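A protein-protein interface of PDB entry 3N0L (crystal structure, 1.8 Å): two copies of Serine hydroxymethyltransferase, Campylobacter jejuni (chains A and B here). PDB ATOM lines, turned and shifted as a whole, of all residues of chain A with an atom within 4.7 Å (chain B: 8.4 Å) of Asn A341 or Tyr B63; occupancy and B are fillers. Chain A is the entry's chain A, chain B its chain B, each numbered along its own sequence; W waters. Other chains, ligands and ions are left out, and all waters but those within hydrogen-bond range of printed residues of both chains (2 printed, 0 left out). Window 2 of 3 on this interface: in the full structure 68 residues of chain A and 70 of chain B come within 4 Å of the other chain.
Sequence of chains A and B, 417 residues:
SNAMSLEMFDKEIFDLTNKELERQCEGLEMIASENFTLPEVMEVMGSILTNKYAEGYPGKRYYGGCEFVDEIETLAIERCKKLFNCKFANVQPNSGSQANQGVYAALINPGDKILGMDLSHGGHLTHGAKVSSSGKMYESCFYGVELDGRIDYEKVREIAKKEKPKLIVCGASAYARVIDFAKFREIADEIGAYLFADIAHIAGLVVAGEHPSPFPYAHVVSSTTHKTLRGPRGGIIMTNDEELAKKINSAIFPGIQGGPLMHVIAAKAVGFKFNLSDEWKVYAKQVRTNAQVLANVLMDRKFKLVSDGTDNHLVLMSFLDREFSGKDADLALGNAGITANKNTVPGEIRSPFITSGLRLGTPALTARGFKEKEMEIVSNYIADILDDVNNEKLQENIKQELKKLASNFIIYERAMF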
ATOM      1  N   ILE A  31       7.981  32.079  -8.435  1.00  0.00           N
ATOM      2  CA  ILE A  31       7.553  31.050  -9.380  1.00  0.00           C
ATOM      3  C   ILE A  31       6.289  31.574 -10.060  1.00  0.00           C
ATOM      4  O   ILE A  31       5.291  31.857  -9.397  1.00  0.00           O
ATOM      5  CB  ILE A  31       7.274  29.719  -8.679  1.00  0.00           C
ATOM      6  CG1 ILE A  31       8.584  29.127  -8.139  1.00  0.00           C
ATOM      7  CG2 ILE A  31       6.546  28.729  -9.617  1.00  0.00           C
ATOM      8  CD1 ILE A  31       8.374  27.918  -7.254  1.00  0.00           C
ATOM      9  N   SER A  33       3.845  30.513 -11.516  1.00  0.00           N
ATOM     10  CA  SER A  33       2.590  29.808 -11.367  1.00  0.00           C
ATOM     11  C   SER A  33       2.139  29.731  -9.911  1.00  0.00           C
ATOM     12  O   SER A  33       1.147  29.075  -9.601  1.00  0.00           O
ATOM     13  CB  SER A  33       2.706  28.406 -11.960  1.00  0.00           C
ATOM     14  OG  SER A  33       3.693  27.675 -11.255  1.00  0.00           O
ATOM     15  N   ASP A 330      18.886  29.523 -10.575  1.00  0.00           N
ATOM     16  CA  ASP A 330      17.794  29.114  -9.703  1.00  0.00           C
ATOM     17  C   ASP A 330      18.293  28.841  -8.284  1.00  0.00           C
ATOM     18  O   ASP A 330      17.679  29.269  -7.298  1.00  0.00           O
ATOM     19  CB  ASP A 330      17.125  27.869 -10.283  1.00  0.00           C
ATOM     20  CG  ASP A 330      15.831  27.517  -9.579  1.00  0.00           C
ATOM     21  OD1 ASP A 330      15.121  28.440  -9.132  1.00  0.00           O
ATOM     22  OD2 ASP A 330      15.516  26.315  -9.486  1.00  0.00           O
ATOM     23  N   ALA A 340      12.210  30.657  -7.624  1.00  0.00           N
ATOM     24  CA  ALA A 340      11.936  30.800  -9.047  1.00  0.00           C
ATOM     25  C   ALA A 340      12.093  29.411  -9.624  1.00  0.00           C
ATOM     26  O   ALA A 340      12.131  28.438  -8.878  1.00  0.00           O
ATOM     27  CB  ALA A 340      12.933  31.755  -9.673  1.00  0.00           C
ATOM     28  N   ASN A 341      12.185  29.287 -10.940  1.00  0.00           N
ATOM     29  CA  ASN A 341      12.559  27.992 -11.501  1.00  0.00           C
ATOM     30  C   ASN A 341      13.345  28.091 -12.795  1.00  0.00           C
ATOM     31  O   ASN A 341      13.111  28.978 -13.608  1.00  0.00           O
ATOM     32  CB  ASN A 341      11.349  27.058 -11.663  1.00  0.00           C
ATOM     33  CG  ASN A 341      10.337  27.570 -12.665  1.00  0.00           C
ATOM     34  OD1 ASN A 341       9.340  28.188 -12.291  1.00  0.00           O
ATOM     35  ND2 ASN A 341      10.576  27.299 -13.947  1.00  0.00           N
ATOM     36  N   LYS A 342      14.288  27.172 -12.970  1.00  0.00           N
ATOM     37  CA  LYS A 342      15.048  27.095 -14.209  1.00  0.00           C
ATOM     38  C   LYS A 342      14.085  26.729 -15.315  1.00  0.00           C
ATOM     39  O   LYS A 342      13.043  26.123 -15.068  1.00  0.00           O
ATOM     40  CB  LYS A 342      16.161  26.052 -14.094  1.00  0.00           C
ATOM     41  CG  LYS A 342      15.663  24.626 -13.983  1.00  0.00           C
ATOM     42  CD  LYS A 342      16.824  23.674 -13.644  1.00  0.00           C
ATOM     43  CE  LYS A 342      16.345  22.243 -13.496  1.00  0.00           C
ATOM     44  NZ  LYS A 342      15.651  22.044 -12.201  1.00  0.00           N
ATOM     45  N   ASN A 343      14.406  27.127 -16.538  1.00  0.00           N
ATOM     46  CA  ASN A 343      13.503  26.910 -17.651  1.00  0.00           C
ATOM     47  C   ASN A 343      14.319  26.906 -18.925  1.00  0.00           C
ATOM     48  O   ASN A 343      15.264  27.687 -19.048  1.00  0.00           O
ATOM     49  CB  ASN A 343      12.479  28.052 -17.704  1.00  0.00           C
ATOM     50  CG  ASN A 343      11.176  27.644 -18.350  1.00  0.00           C
ATOM     51  OD1 ASN A 343      10.198  27.362 -17.660  1.00  0.00           O
ATOM     52  ND2 ASN A 343      11.148  27.622 -19.682  1.00  0.00           N
ATOM     53  N   GLY A 357      17.961  29.056 -18.853  1.00  0.00           N
ATOM     54  CA  GLY A 357      17.052  30.146 -18.567  1.00  0.00           C
ATOM     55  C   GLY A 357      16.427  30.097 -17.187  1.00  0.00           C
ATOM     56  O   GLY A 357      16.648  29.163 -16.408  1.00  0.00           O
ATOM     57  N   LEU A 358      15.637  31.123 -16.893  1.00  0.00           N
ATOM     58  CA  LEU A 358      15.009  31.268 -15.595  1.00  0.00           C
ATOM     59  C   LEU A 358      13.651  31.922 -15.770  1.00  0.00           C
ATOM     60  O   LEU A 358      13.546  33.002 -16.349  1.00  0.00           O
ATOM     61  CB  LEU A 358      15.890  32.125 -14.685  1.00  0.00           C
ATOM     62  CG  LEU A 358      15.445  32.234 -13.228  1.00  0.00           C
ATOM     63  CD1 LEU A 358      15.723  30.920 -12.496  1.00  0.00           C
ATOM     64  CD2 LEU A 358      16.161  33.405 -12.554  1.00  0.00           C
ATOM     65  N   ARG A 359      12.604  31.267 -15.290  1.00  0.00           N
ATOM     66  CA  ARG A 359      11.279  31.874 -15.353  1.00  0.00           C
ATOM     67  C   ARG A 359      10.961  32.587 -14.048  1.00  0.00           C
ATOM     68  O   ARG A 359      11.192  32.036 -12.977  1.00  0.00           O
ATOM     69  CB  ARG A 359      10.203  30.825 -15.630  1.00  0.00           C
ATOM     70  CG  ARG A 359       8.831  31.439 -15.845  1.00  0.00           C
ATOM     71  CD  ARG A 359       7.765  30.368 -15.982  1.00  0.00           C
ATOM     72  NE  ARG A 359       7.666  29.567 -14.763  1.00  0.00           N
ATOM     73  CZ  ARG A 359       6.735  28.642 -14.556  1.00  0.00           C
ATOM     74  NH1 ARG A 359       5.807  28.422 -15.477  1.00  0.00           N
ATOM     75  NH2 ARG A 359       6.714  27.958 -13.418  1.00  0.00           N
ATOM     76  N   LYS B  52       1.177  25.693  -2.001  1.00  0.00           N
ATOM     77  CA  LYS B  52       2.443  25.079  -2.394  1.00  0.00           C
ATOM     78  C   LYS B  52       2.283  24.207  -3.634  1.00  0.00           C
ATOM     79  O   LYS B  52       1.426  23.331  -3.680  1.00  0.00           O
ATOM     80  CB  LYS B  52       3.045  24.277  -1.234  1.00  0.00           C
ATOM     81  CG  LYS B  52       4.488  23.820  -1.476  1.00  0.00           C
ATOM     82  CD  LYS B  52       5.375  24.974  -1.882  1.00  0.00           C
ATOM     83  CE  LYS B  52       6.780  24.495  -2.241  1.00  0.00           C
ATOM     84  NZ  LYS B  52       7.496  25.486  -3.094  1.00  0.00           N
ATOM     85  N   TYR B  53       3.094  24.471  -4.655  1.00  0.00           N
ATOM     86  CA  TYR B  53       3.099  23.635  -5.846  1.00  0.00           C
ATOM     87  C   TYR B  53       4.273  22.663  -5.732  1.00  0.00           C
ATOM     88  O   TYR B  53       5.436  23.059  -5.823  1.00  0.00           O
ATOM     89  CB  TYR B  53       3.213  24.491  -7.113  1.00  0.00           C
ATOM     90  CG  TYR B  53       2.725  23.781  -8.358  1.00  0.00           C
ATOM     91  CD1 TYR B  53       1.876  22.687  -8.267  1.00  0.00           C
ATOM     92  CD2 TYR B  53       3.123  24.197  -9.624  1.00  0.00           C
ATOM     93  CE1 TYR B  53       1.429  22.028  -9.398  1.00  0.00           C
ATOM     94  CE2 TYR B  53       2.680  23.542 -10.763  1.00  0.00           C
ATOM     95  CZ  TYR B  53       1.834  22.458 -10.640  1.00  0.00           C
ATOM     96  OH  TYR B  53       1.384  21.799 -11.762  1.00  0.00           O
ATOM     97  N   ALA B  54       3.969  21.394  -5.497  1.00  0.00           N
ATOM     98  CA  ALA B  54       5.020  20.427  -5.208  1.00  0.00           C
ATOM     99  C   ALA B  54       5.056  19.237  -6.170  1.00  0.00           C
ATOM    100  O   ALA B  54       5.019  18.085  -5.735  1.00  0.00           O
ATOM    101  CB  ALA B  54       4.911  19.943  -3.758  1.00  0.00           C
ATOM    102  N   GLU B  55       5.163  19.511  -7.467  1.00  0.00           N
ATOM    103  CA  GLU B  55       5.296  18.429  -8.446  1.00  0.00           C
ATOM    104  C   GLU B  55       6.516  17.553  -8.160  1.00  0.00           C
ATOM    105  O   GLU B  55       7.584  18.058  -7.804  1.00  0.00           O
ATOM    106  CB  GLU B  55       5.379  18.978  -9.875  1.00  0.00           C
ATOM    107  CG  GLU B  55       4.092  19.599 -10.374  1.00  0.00           C
ATOM    108  CD  GLU B  55       4.150  19.939 -11.856  1.00  0.00           C
ATOM    109  OE1 GLU B  55       5.208  20.422 -12.315  1.00  0.00           O
ATOM    110  OE2 GLU B  55       3.141  19.708 -12.559  1.00  0.00           O
ATOM    111  N   GLY B  56       6.353  16.245  -8.337  1.00  0.00           N
ATOM    112  CA  GLY B  56       7.413  15.293  -8.035  1.00  0.00           C
ATOM    113  C   GLY B  56       7.164  14.609  -6.702  1.00  0.00           C
ATOM    114  O   GLY B  56       6.054  14.659  -6.183  1.00  0.00           O
ATOM    115  N   TYR B  57       8.189  13.967  -6.148  1.00  0.00           N
ATOM    116  CA  TYR B  57       8.051  13.252  -4.875  1.00  0.00           C
ATOM    117  C   TYR B  57       9.034  13.824  -3.849  1.00  0.00           C
ATOM    118  O   TYR B  57       9.902  14.628  -4.201  1.00  0.00           O
ATOM    119  CB  TYR B  57       8.221  11.731  -5.087  1.00  0.00           C
ATOM    120  CG  TYR B  57       7.072  11.157  -5.898  1.00  0.00           C
ATOM    121  CD1 TYR B  57       5.876  10.830  -5.284  1.00  0.00           C
ATOM    122  CD2 TYR B  57       7.159  11.020  -7.284  1.00  0.00           C
ATOM    123  CE1 TYR B  57       4.795  10.345  -6.015  1.00  0.00           C
ATOM    124  CE2 TYR B  57       6.085  10.534  -8.029  1.00  0.00           C
ATOM    125  CZ  TYR B  57       4.904  10.189  -7.378  1.00  0.00           C
ATOM    126  OH  TYR B  57       3.826   9.708  -8.083  1.00  0.00           O
ATOM    127  N   GLY B  59      12.015  14.893  -1.729  1.00  0.00           N
ATOM    128  CA  GLY B  59      13.428  14.841  -2.059  1.00  0.00           C
ATOM    129  C   GLY B  59      13.706  14.837  -3.549  1.00  0.00           C
ATOM    130  O   GLY B  59      14.863  14.819  -3.965  1.00  0.00           O
ATOM    131  N   LYS B  60      12.647  14.865  -4.354  1.00  0.00           N
ATOM    132  CA  LYS B  60      12.765  14.784  -5.808  1.00  0.00           C
ATOM    133  C   LYS B  60      11.729  15.679  -6.474  1.00  0.00           C
ATOM    134  O   LYS B  60      11.005  15.251  -7.378  1.00  0.00           O
ATOM    135  CB  LYS B  60      12.559  13.343  -6.279  1.00  0.00           C
ATOM    136  CG  LYS B  60      13.612  12.365  -5.783  1.00  0.00           C
ATOM    137  CD  LYS B  60      13.153  10.924  -5.965  1.00  0.00           C
ATOM    138  CE  LYS B  60      14.262   9.943  -5.615  1.00  0.00           C
ATOM    139  NZ  LYS B  60      14.822  10.185  -4.254  1.00  0.00           N
ATOM    140  N   ARG B  61      11.654  16.923  -6.020  1.00  0.00           N
ATOM    141  CA  ARG B  61      10.649  17.850  -6.521  1.00  0.00           C
ATOM    142  C   ARG B  61      11.179  18.652  -7.698  1.00  0.00           C
ATOM    143  O   ARG B  61      12.384  18.821  -7.851  1.00  0.00           O
ATOM    144  CB  ARG B  61      10.256  18.818  -5.414  1.00  0.00           C
ATOM    145  CG  ARG B  61       9.767  18.152  -4.160  1.00  0.00           C
ATOM    146  CD  ARG B  61       8.337  17.647  -4.289  1.00  0.00           C
ATOM    147  NE  ARG B  61       7.828  17.371  -2.952  1.00  0.00           N
ATOM    148  CZ  ARG B  61       6.745  16.655  -2.669  1.00  0.00           C
ATOM    149  NH1 ARG B  61       6.009  16.119  -3.635  1.00  0.00           N
ATOM    150  NH2 ARG B  61       6.398  16.484  -1.401  1.00  0.00           N
ATOM    151  N   TYR B  62      10.271  19.173  -8.514  1.00  0.00           N
ATOM    152  CA  TYR B  62      10.671  20.028  -9.625  1.00  0.00           C
ATOM    153  C   TYR B  62      11.051  21.440  -9.177  1.00  0.00           C
ATOM    154  O   TYR B  62      11.920  22.067  -9.775  1.00  0.00           O
ATOM    155  CB  TYR B  62       9.585  20.060 -10.707  1.00  0.00           C
ATOM    156  CG  TYR B  62       9.507  18.771 -11.500  1.00  0.00           C
ATOM    157  CD1 TYR B  62      10.026  17.585 -10.987  1.00  0.00           C
ATOM    158  CD2 TYR B  62       8.941  18.742 -12.770  1.00  0.00           C
ATOM    159  CE1 TYR B  62       9.970  16.406 -11.703  1.00  0.00           C
ATOM    160  CE2 TYR B  62       8.880  17.564 -13.498  1.00  0.00           C
ATOM    161  CZ  TYR B  62       9.396  16.399 -12.958  1.00  0.00           C
ATOM    162  OH  TYR B  62       9.341  15.221 -13.674  1.00  0.00           O
ATOM    163  N   TYR B  63      10.410  21.933  -8.122  1.00  0.00           N
ATOM    164  CA  TYR B  63      10.703  23.269  -7.601  1.00  0.00           C
ATOM    165  C   TYR B  63      11.383  23.202  -6.245  1.00  0.00           C
ATOM    166  O   TYR B  63      11.299  22.188  -5.551  1.00  0.00           O
ATOM    167  CB  TYR B  63       9.415  24.075  -7.444  1.00  0.00           C
ATOM    168  CG  TYR B  63       8.660  24.304  -8.728  1.00  0.00           C
ATOM    169  CD1 TYR B  63       9.316  24.716  -9.878  1.00  0.00           C
ATOM    170  CD2 TYR B  63       7.290  24.099  -8.791  1.00  0.00           C
ATOM    171  CE1 TYR B  63       8.622  24.924 -11.055  1.00  0.00           C
ATOM    172  CE2 TYR B  63       6.591  24.301  -9.960  1.00  0.00           C
ATOM    173  CZ  TYR B  63       7.260  24.715 -11.087  1.00  0.00           C
ATOM    174  OH  TYR B  63       6.560  24.916 -12.250  1.00  0.00           O
ATOM    175  N   GLY B  64      12.030  24.302  -5.865  1.00  0.00           N
ATOM    176  CA  GLY B  64      12.617  24.441  -4.544  1.00  0.00           C
ATOM    177  C   GLY B  64      11.599  24.872  -3.499  1.00  0.00           C
ATOM    178  O   GLY B  64      10.436  25.115  -3.821  1.00  0.00           O
ATOM    179  N   GLY B  65      12.035  24.956  -2.244  1.00  0.00           N
ATOM    180  CA  GLY B  65      11.182  25.418  -1.162  1.00  0.00           C
ATOM    181  C   GLY B  65      10.270  24.349  -0.588  1.00  0.00           C
ATOM    182  O   GLY B  65       9.280  24.663   0.074  1.00  0.00           O
ATOM    183  N   CYS B  66      10.604  23.083  -0.824  1.00  0.00           N
ATOM    184  CA  CYS B  66       9.718  21.984  -0.438  1.00  0.00           C
ATOM    185  C   CYS B  66      10.135  21.264   0.842  1.00  0.00           C
ATOM    186  O   CYS B  66       9.651  20.167   1.115  1.00  0.00           O
ATOM    187  CB  CYS B  66       9.590  20.959  -1.571  1.00  0.00           C
ATOM    188  SG  CYS B  66       8.677  21.549  -3.020  1.00  0.00           S
ATOM    189  N   GLU B  67      11.006  21.883   1.635  1.00  0.00           N
ATOM    190  CA  GLU B  67      11.526  21.233   2.833  1.00  0.00           C
ATOM    191  C   GLU B  67      10.406  20.691   3.716  1.00  0.00           C
ATOM    192  O   GLU B  67      10.441  19.541   4.150  1.00  0.00           O
ATOM    193  CB  GLU B  67      12.395  22.203   3.649  1.00  0.00           C
ATOM    194  CG  GLU B  67      13.025  21.567   4.887  1.00  0.00           C
ATOM    195  CD  GLU B  67      13.817  22.554   5.743  1.00  0.00           C
ATOM    196  OE1 GLU B  67      13.892  23.751   5.385  1.00  0.00           O
ATOM    197  OE2 GLU B  67      14.362  22.123   6.786  1.00  0.00           O
ATOM    198  N   VAL B  69       6.897  20.582   3.080  1.00  0.00           N
ATOM    199  CA  VAL B  69       5.887  19.727   2.463  1.00  0.00           C
ATOM    200  C   VAL B  69       6.449  18.316   2.198  1.00  0.00           C
ATOM    201  O   VAL B  69       5.702  17.341   2.176  1.00  0.00           O
ATOM    202  CB  VAL B  69       5.267  20.334   1.178  1.00  0.00           C
ATOM    203  CG1 VAL B  69       4.529  21.638   1.501  1.00  0.00           C
ATOM    204  CG2 VAL B  69       6.329  20.558   0.114  1.00  0.00           C
ATOM    205  N   ASP B  70       7.758  18.210   1.980  1.00  0.00           N
ATOM    206  CA  ASP B  70       8.385  16.895   1.838  1.00  0.00           C
ATOM    207  C   ASP B  70       8.259  16.114   3.147  1.00  0.00           C
ATOM    208  O   ASP B  70       7.986  14.914   3.144  1.00  0.00           O
ATOM    209  CB  ASP B  70       9.863  17.012   1.456  1.00  0.00           C
ATOM    210  CG  ASP B  70      10.061  17.378  -0.002  1.00  0.00           C
ATOM    211  OD1 ASP B  70       9.050  17.601  -0.702  1.00  0.00           O
ATOM    212  OD2 ASP B  70      11.232  17.453  -0.448  1.00  0.00           O
ATOM    213  N   GLY B 259       0.960  18.606  -9.907  1.00  0.00           N
ATOM    214  CA  GLY B 259       1.225  18.781  -8.493  1.00  0.00           C
ATOM    215  C   GLY B 259       0.102  18.224  -7.633  1.00  0.00           C
ATOM    216  O   GLY B 259      -1.074  18.323  -7.975  1.00  0.00           O
HETATM  217  O   HOH W   1      12.954  26.089  -8.074  1.00  0.00           O
HETATM  218  O   HOH W   2      13.638  24.526 -10.785  1.00  0.00           O
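NH2 of Arg A359 lies within hydrogen-bond range of OH of Tyr B63, 3.3 Å away.
The side-chain amide oxygen (OD1) of Asn A341 sits at hydrogen-bond distance from the guanidinium group (NH2) of Arg A359, 2.9 Å away.
OH of Tyr B53 lies within hydrogen-bond range of OE2 of Glu B55.
The backbone carbonyl oxygen (O) of Tyr B63 lies within hydrogen-bond range of the side-chain sulfur (SG) of Cys B66 (3.7 Å).
Among the printed residues, merely in contact across the chains: Asn A341 with Tyr B63, Ser A33 with Tyr B53 and Ile A31 with Tyr B63.
Of the printed residues of chain B, Ile A31 touches Tyr B63 (3.9 Å).
Of the printed residues of chain B, Ser A33 touches Tyr B53 (3.9 Å).
No residue of chain B comes within 4 Å of Ala A340.
Of chain B, only Tyr B63 comes within 4 Å of Asn A341.
Asn A343 touches none of the printed residues of chain B.
Printed residues of chain A within 4 Å of Tyr B53: Ser A33.
Tyr B63 touches just these residues of chain A: Ile A31, Asn A341 and Arg A359.
The nearest residue of chain A that does not touch Tyr B63 is Ser A33 (4.1 Å).
The nearest printed residue of chain B that does not touch Ser A33 is Tyr B63 (4.1 Å).
Of the 18 printed residues of chain B, 2 touch a printed residue of chain A.
Printed residues of chain B that touch a printed residue of chain A: Tyr B53 and Tyr B63.
Hydrophobic or aromatic side chains of chain B within 4 Å of the printed part of chain A: Tyr B53 and Tyr B63.
Along chain B the printed residues that touch a printed residue of chain A span positions 53 to 63.
Of the 10 printed residues of chain A, 4 touch a printed residue of chain B.
Among the printed residues, no Asp or Glu carboxylate lies within 4 Å of a Lys or Arg side-chain nitrogen of the other chain.
No position is printed for both chains.
Water W1 lies within hydrogen-bond range of the backbone carbonyl oxygen of Ala A340 (2.6 Å), the side-chain carboxylate of Asp A330 (2.9 Å) and the backbone NH of Gly B64 (3.0 Å).
Water W2 lies within hydrogen-bond range of OD2 of Asp A330, O of Tyr B62 and N of Lys A342.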
